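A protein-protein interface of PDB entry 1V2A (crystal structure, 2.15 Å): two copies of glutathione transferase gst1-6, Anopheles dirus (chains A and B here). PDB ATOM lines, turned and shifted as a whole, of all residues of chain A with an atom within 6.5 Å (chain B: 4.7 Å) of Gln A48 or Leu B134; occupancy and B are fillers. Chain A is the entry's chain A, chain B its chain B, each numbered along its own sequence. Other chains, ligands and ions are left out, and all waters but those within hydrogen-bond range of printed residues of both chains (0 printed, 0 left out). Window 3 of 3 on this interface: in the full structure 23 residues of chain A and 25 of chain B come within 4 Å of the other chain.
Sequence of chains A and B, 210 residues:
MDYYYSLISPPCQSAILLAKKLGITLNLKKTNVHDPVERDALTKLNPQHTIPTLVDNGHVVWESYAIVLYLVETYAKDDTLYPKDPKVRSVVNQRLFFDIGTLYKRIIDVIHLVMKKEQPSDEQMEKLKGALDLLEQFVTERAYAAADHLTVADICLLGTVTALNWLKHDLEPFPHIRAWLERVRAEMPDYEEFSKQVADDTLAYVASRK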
ATOM      1  N   LEU A  42      29.265  16.694  -1.470  1.00  0.00           N
ATOM      2  CA  LEU A  42      27.941  16.285  -1.927  1.00  0.00           C
ATOM      3  C   LEU A  42      26.899  17.174  -1.268  1.00  0.00           C
ATOM      4  O   LEU A  42      25.944  17.618  -1.908  1.00  0.00           O
ATOM      5  CB  LEU A  42      27.671  14.822  -1.550  1.00  0.00           C
ATOM      6  CG  LEU A  42      26.675  13.995  -2.386  1.00  0.00           C
ATOM      7  CD1 LEU A  42      25.809  13.172  -1.441  1.00  0.00           C
ATOM      8  CD2 LEU A  42      25.797  14.878  -3.261  1.00  0.00           C
ATOM      9  N   THR A  43      27.096  17.421   0.023  1.00  0.00           N
ATOM     10  CA  THR A  43      26.192  18.249   0.809  1.00  0.00           C
ATOM     11  C   THR A  43      26.123  19.675   0.277  1.00  0.00           C
ATOM     12  O   THR A  43      25.064  20.299   0.308  1.00  0.00           O
ATOM     13  CB  THR A  43      26.638  18.284   2.276  1.00  0.00           C
ATOM     14  OG1 THR A  43      26.578  16.960   2.821  1.00  0.00           O
ATOM     15  CG2 THR A  43      25.740  19.207   3.089  1.00  0.00           C
ATOM     16  N   ASN A  46      23.673  18.914  -2.432  1.00  0.00           N
ATOM     17  CA  ASN A  46      22.440  18.352  -1.913  1.00  0.00           C
ATOM     18  C   ASN A  46      22.623  18.228  -0.398  1.00  0.00           C
ATOM     19  O   ASN A  46      23.367  17.366   0.071  1.00  0.00           O
ATOM     20  CB  ASN A  46      22.227  16.975  -2.549  1.00  0.00           C
ATOM     21  CG  ASN A  46      21.126  16.178  -1.885  1.00  0.00           C
ATOM     22  OD1 ASN A  46      20.955  14.987  -2.163  1.00  0.00           O
ATOM     23  ND2 ASN A  46      20.370  16.825  -1.006  1.00  0.00           N
ATOM     24  N   PRO A  47      21.948  19.092   0.385  1.00  0.00           N
ATOM     25  CA  PRO A  47      22.036  19.087   1.851  1.00  0.00           C
ATOM     26  C   PRO A  47      21.595  17.784   2.519  1.00  0.00           C
ATOM     27  O   PRO A  47      22.024  17.481   3.632  1.00  0.00           O
ATOM     28  CB  PRO A  47      21.156  20.268   2.251  1.00  0.00           C
ATOM     29  CG  PRO A  47      20.118  20.288   1.161  1.00  0.00           C
ATOM     30  CD  PRO A  47      20.963  20.088  -0.074  1.00  0.00           C
ATOM     31  N   GLN A  48      20.729  17.021   1.865  1.00  0.00           N
ATOM     32  CA  GLN A  48      20.301  15.762   2.462  1.00  0.00           C
ATOM     33  C   GLN A  48      21.403  14.741   2.231  1.00  0.00           C
ATOM     34  O   GLN A  48      21.398  13.648   2.808  1.00  0.00           O
ATOM     35  CB  GLN A  48      18.984  15.265   1.852  1.00  0.00           C
ATOM     36  CG  GLN A  48      18.385  14.098   2.645  1.00  0.00           C
ATOM     37  CD  GLN A  48      16.990  13.709   2.206  1.00  0.00           C
ATOM     38  OE1 GLN A  48      16.417  12.755   2.726  1.00  0.00           O
ATOM     39  NE2 GLN A  48      16.435  14.443   1.251  1.00  0.00           N
ATOM     40  N   HIS A  49      22.360  15.128   1.393  1.00  0.00           N
ATOM     41  CA  HIS A  49      23.504  14.295   1.036  1.00  0.00           C
ATOM     42  C   HIS A  49      23.163  12.827   0.812  1.00  0.00           C
ATOM     43  O   HIS A  49      23.658  11.945   1.519  1.00  0.00           O
ATOM     44  CB  HIS A  49      24.634  14.432   2.083  1.00  0.00           C
ATOM     45  CG  HIS A  49      24.221  14.116   3.489  1.00  0.00           C
ATOM     46  ND1 HIS A  49      23.926  12.838   3.913  1.00  0.00           N
ATOM     47  CD2 HIS A  49      24.044  14.919   4.565  1.00  0.00           C
ATOM     48  CE1 HIS A  49      23.583  12.869   5.190  1.00  0.00           C
ATOM     49  NE2 HIS A  49      23.647  14.119   5.608  1.00  0.00           N
ATOM     50  N   THR A  50      22.308  12.580  -0.178  1.00  0.00           N
ATOM     51  CA  THR A  50      21.923  11.220  -0.535  1.00  0.00           C
ATOM     52  C   THR A  50      22.150  11.008  -2.024  1.00  0.00           C
ATOM     53  O   THR A  50      22.167  11.963  -2.805  1.00  0.00           O
ATOM     54  CB  THR A  50      20.424  10.921  -0.275  1.00  0.00           C
ATOM     55  OG1 THR A  50      19.618  11.790  -1.079  1.00  0.00           O
ATOM     56  CG2 THR A  50      20.065  11.107   1.188  1.00  0.00           C
ATOM     57  N   TRP A  62      17.806  15.822  -6.805  1.00  0.00           N
ATOM     58  CA  TRP A  62      18.037  14.593  -6.058  1.00  0.00           C
ATOM     59  C   TRP A  62      16.695  13.928  -5.809  1.00  0.00           C
ATOM     60  O   TRP A  62      15.648  14.571  -5.929  1.00  0.00           O
ATOM     61  CB  TRP A  62      18.849  14.839  -4.782  1.00  0.00           C
ATOM     62  CG  TRP A  62      18.159  15.470  -3.634  1.00  0.00           C
ATOM     63  CD1 TRP A  62      17.517  14.832  -2.613  1.00  0.00           C
ATOM     64  CD2 TRP A  62      18.130  16.864  -3.322  1.00  0.00           C
ATOM     65  NE1 TRP A  62      17.100  15.744  -1.677  1.00  0.00           N
ATOM     66  CE2 TRP A  62      17.463  17.001  -2.089  1.00  0.00           C
ATOM     67  CE3 TRP A  62      18.608  18.013  -3.965  1.00  0.00           C
ATOM     68  CZ2 TRP A  62      17.262  18.245  -1.478  1.00  0.00           C
ATOM     69  CZ3 TRP A  62      18.407  19.254  -3.357  1.00  0.00           C
ATOM     70  CH2 TRP A  62      17.740  19.356  -2.128  1.00  0.00           C
ATOM     71  N   GLU A  63      16.749  12.637  -5.490  1.00  0.00           N
ATOM     72  CA  GLU A  63      15.586  11.769  -5.329  1.00  0.00           C
ATOM     73  C   GLU A  63      15.474  11.153  -6.735  1.00  0.00           C
ATOM     74  O   GLU A  63      15.117  11.841  -7.700  1.00  0.00           O
ATOM     75  CB  GLU A  63      14.301  12.545  -5.013  1.00  0.00           C
ATOM     76  CG  GLU A  63      14.055  12.856  -3.539  1.00  0.00           C
ATOM     77  CD  GLU A  63      13.850  11.617  -2.692  1.00  0.00           C
ATOM     78  OE1 GLU A  63      13.247  10.642  -3.185  1.00  0.00           O
ATOM     79  OE2 GLU A  63      14.278  11.614  -1.519  1.00  0.00           O
ATOM     80  N   PHE B  98      10.334  14.027  -0.820  1.00  0.00           N
ATOM     81  CA  PHE B  98      10.951  14.279   0.472  1.00  0.00           C
ATOM     82  C   PHE B  98       9.849  14.081   1.518  1.00  0.00           C
ATOM     83  O   PHE B  98      10.069  13.520   2.591  1.00  0.00           O
ATOM     84  CB  PHE B  98      11.452  15.725   0.528  1.00  0.00           C
ATOM     85  CG  PHE B  98      11.715  16.220   1.919  1.00  0.00           C
ATOM     86  CD1 PHE B  98      12.833  15.790   2.625  1.00  0.00           C
ATOM     87  CD2 PHE B  98      10.831  17.100   2.534  1.00  0.00           C
ATOM     88  CE1 PHE B  98      13.064  16.232   3.924  1.00  0.00           C
ATOM     89  CE2 PHE B  98      11.053  17.544   3.822  1.00  0.00           C
ATOM     90  CZ  PHE B  98      12.168  17.113   4.522  1.00  0.00           C
ATOM     91  N   THR B 102      10.532  10.947   3.410  1.00  0.00           N
ATOM     92  CA  THR B 102      11.466  11.397   4.430  1.00  0.00           C
ATOM     93  C   THR B 102      10.790  11.949   5.667  1.00  0.00           C
ATOM     94  O   THR B 102      10.831  11.328   6.725  1.00  0.00           O
ATOM     95  CB  THR B 102      12.424  12.473   3.884  1.00  0.00           C
ATOM     96  OG1 THR B 102      13.180  11.926   2.796  1.00  0.00           O
ATOM     97  CG2 THR B 102      13.381  12.950   4.979  1.00  0.00           C
ATOM     98  N   GLY B 130      16.416  15.288  11.891  1.00  0.00           N
ATOM     99  CA  GLY B 130      17.133  15.458  10.639  1.00  0.00           C
ATOM    100  C   GLY B 130      16.236  15.913   9.504  1.00  0.00           C
ATOM    101  O   GLY B 130      16.607  16.799   8.733  1.00  0.00           O
ATOM    102  N   ALA B 131      15.050  15.315   9.399  1.00  0.00           N
ATOM    103  CA  ALA B 131      14.124  15.675   8.337  1.00  0.00           C
ATOM    104  C   ALA B 131      13.655  17.116   8.500  1.00  0.00           C
ATOM    105  O   ALA B 131      13.509  17.848   7.523  1.00  0.00           O
ATOM    106  CB  ALA B 131      12.938  14.733   8.346  1.00  0.00           C
ATOM    107  N   LEU B 132      13.435  17.518   9.747  1.00  0.00           N
ATOM    108  CA  LEU B 132      12.971  18.864  10.045  1.00  0.00           C
ATOM    109  C   LEU B 132      14.026  19.914   9.722  1.00  0.00           C
ATOM    110  O   LEU B 132      13.713  20.959   9.138  1.00  0.00           O
ATOM    111  CB  LEU B 132      12.559  18.959  11.518  1.00  0.00           C
ATOM    112  CG  LEU B 132      11.473  17.970  11.957  1.00  0.00           C
ATOM    113  CD1 LEU B 132      11.233  18.109  13.449  1.00  0.00           C
ATOM    114  CD2 LEU B 132      10.189  18.227  11.180  1.00  0.00           C
ATOM    115  N   ASP B 133      15.275  19.641  10.098  1.00  0.00           N
ATOM    116  CA  ASP B 133      16.355  20.580   9.816  1.00  0.00           C
ATOM    117  C   ASP B 133      16.407  20.830   8.317  1.00  0.00           C
ATOM    118  O   ASP B 133      16.658  21.949   7.864  1.00  0.00           O
ATOM    119  CB  ASP B 133      17.703  20.026  10.289  1.00  0.00           C
ATOM    120  CG  ASP B 133      17.783  19.894  11.795  1.00  0.00           C
ATOM    121  OD1 ASP B 133      17.371  20.848  12.490  1.00  0.00           O
ATOM    122  OD2 ASP B 133      18.264  18.847  12.282  1.00  0.00           O
ATOM    123  N   LEU B 134      16.175  19.774   7.545  1.00  0.00           N
ATOM    124  CA  LEU B 134      16.182  19.892   6.096  1.00  0.00           C
ATOM    125  C   LEU B 134      15.052  20.811   5.659  1.00  0.00           C
ATOM    126  O   LEU B 134      15.278  21.778   4.922  1.00  0.00           O
ATOM    127  CB  LEU B 134      16.025  18.514   5.450  1.00  0.00           C
ATOM    128  CG  LEU B 134      17.320  17.702   5.348  1.00  0.00           C
ATOM    129  CD1 LEU B 134      17.020  16.274   4.917  1.00  0.00           C
ATOM    130  CD2 LEU B 134      18.250  18.385   4.355  1.00  0.00           C
ATOM    131  N   LEU B 135      13.836  20.509   6.117  1.00  0.00           N
ATOM    132  CA  LEU B 135      12.682  21.332   5.773  1.00  0.00           C
ATOM    133  C   LEU B 135      12.998  22.759   6.216  1.00  0.00           C
ATOM    134  O   LEU B 135      12.752  23.715   5.492  1.00  0.00           O
ATOM    135  CB  LEU B 135      11.417  20.836   6.485  1.00  0.00           C
ATOM    136  CG  LEU B 135      10.142  21.636   6.164  1.00  0.00           C
ATOM    137  CD1 LEU B 135       9.786  21.459   4.684  1.00  0.00           C
ATOM    138  CD2 LEU B 135       8.986  21.172   7.036  1.00  0.00           C
ATOM    139  N   GLU B 136      13.559  22.888   7.410  1.00  0.00           N
ATOM    140  CA  GLU B 136      13.919  24.194   7.935  1.00  0.00           C
ATOM    141  C   GLU B 136      14.793  24.917   6.906  1.00  0.00           C
ATOM    142  O   GLU B 136      14.543  26.078   6.591  1.00  0.00           O
ATOM    143  CB  GLU B 136      14.658  24.032   9.266  1.00  0.00           C
ATOM    144  CG  GLU B 136      15.110  25.332   9.911  1.00  0.00           C
ATOM    145  CD  GLU B 136      13.961  26.208  10.395  1.00  0.00           C
ATOM    146  OE1 GLU B 136      12.802  25.737  10.451  1.00  0.00           O
ATOM    147  OE2 GLU B 136      14.229  27.376  10.737  1.00  0.00           O
ATOM    148  N   GLN B 137      15.802  24.225   6.371  1.00  0.00           N
ATOM    149  CA  GLN B 137      16.689  24.816   5.364  1.00  0.00           C
ATOM    150  C   GLN B 137      15.901  25.191   4.112  1.00  0.00           C
ATOM    151  O   GLN B 137      16.059  26.283   3.579  1.00  0.00           O
ATOM    152  CB  GLN B 137      17.815  23.845   4.975  1.00  0.00           C
ATOM    153  CG  GLN B 137      18.840  23.574   6.075  1.00  0.00           C
ATOM    154  CD  GLN B 137      19.894  22.550   5.669  1.00  0.00           C
ATOM    155  OE1 GLN B 137      20.623  22.747   4.693  1.00  0.00           O
ATOM    156  NE2 GLN B 137      19.982  21.455   6.419  1.00  0.00           N
ATOM    157  N   PHE B 138      15.054  24.281   3.645  1.00  0.00           N
ATOM    158  CA  PHE B 138      14.244  24.533   2.460  1.00  0.00           C
ATOM    159  C   PHE B 138      13.495  25.862   2.568  1.00  0.00           C
ATOM    160  O   PHE B 138      13.541  26.695   1.662  1.00  0.00           O
ATOM    161  CB  PHE B 138      13.228  23.400   2.260  1.00  0.00           C
ATOM    162  CG  PHE B 138      13.852  22.054   1.986  1.00  0.00           C
ATOM    163  CD1 PHE B 138      13.079  20.895   2.045  1.00  0.00           C
ATOM    164  CD2 PHE B 138      15.193  21.944   1.642  1.00  0.00           C
ATOM    165  CE1 PHE B 138      13.639  19.643   1.779  1.00  0.00           C
ATOM    166  CE2 PHE B 138      15.763  20.702   1.375  1.00  0.00           C
ATOM    167  CZ  PHE B 138      14.980  19.549   1.440  1.00  0.00           C
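The side-chain amide oxygen (OE1) of Gln A48 is in hydrogen-bond range of the side-chain hydroxyl (OG1) of Thr B102 (3.3 Å).
ND2 of Asn A46 lies close to N of Gln A48, at 2.9 Å. The indole nitrogen (NE1) of Trp A62 sits close to the side-chain amide nitrogen (NE2) of Gln A48 (3.3 Å).
Among the printed residues, pairs that only touch across the chains: Pro A47 with Leu B134, Pro A47 with Gln B137, Gln A48 with Leu B134 and Trp A62 with Phe B138.
Of chain B, only Thr B102 and Leu B134 come within 4 Å of Gln A48. Printed residues of chain A within 4 Å of Phe B138: Trp A62 (3.9 Å). Of the printed residues of chain A, Thr B102 touches Gln A48. Printed residues of chain B within 4 Å of Pro A47: Leu B134 and Gln B137. His A49 touches none of the printed residues of chain B.
Of the 9 printed residues of chain A, 3 touch a printed residue of chain B. Printed residues of chain A that touch a printed residue of chain B: Pro A47, Gln A48 and Trp A62. Hydrophobic or aromatic side chains of chain A that line the printed part of chain B: Pro A47 and Trp A62. Hydrophobic or aromatic side chains of chain B that line the printed part of chain A: Leu B134 and Phe B138. Along chain B the printed residues that touch a printed residue of chain A span positions 102 to 138. Among the printed residues, no Asp or Glu carboxylate lies within 4 Å of a Lys or Arg side-chain nitrogen of the other chain.
No position is printed for both chains. Of the 5 pairs that touch across the chains among the printed residues, none has its exchanged pair printed and touching as well.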
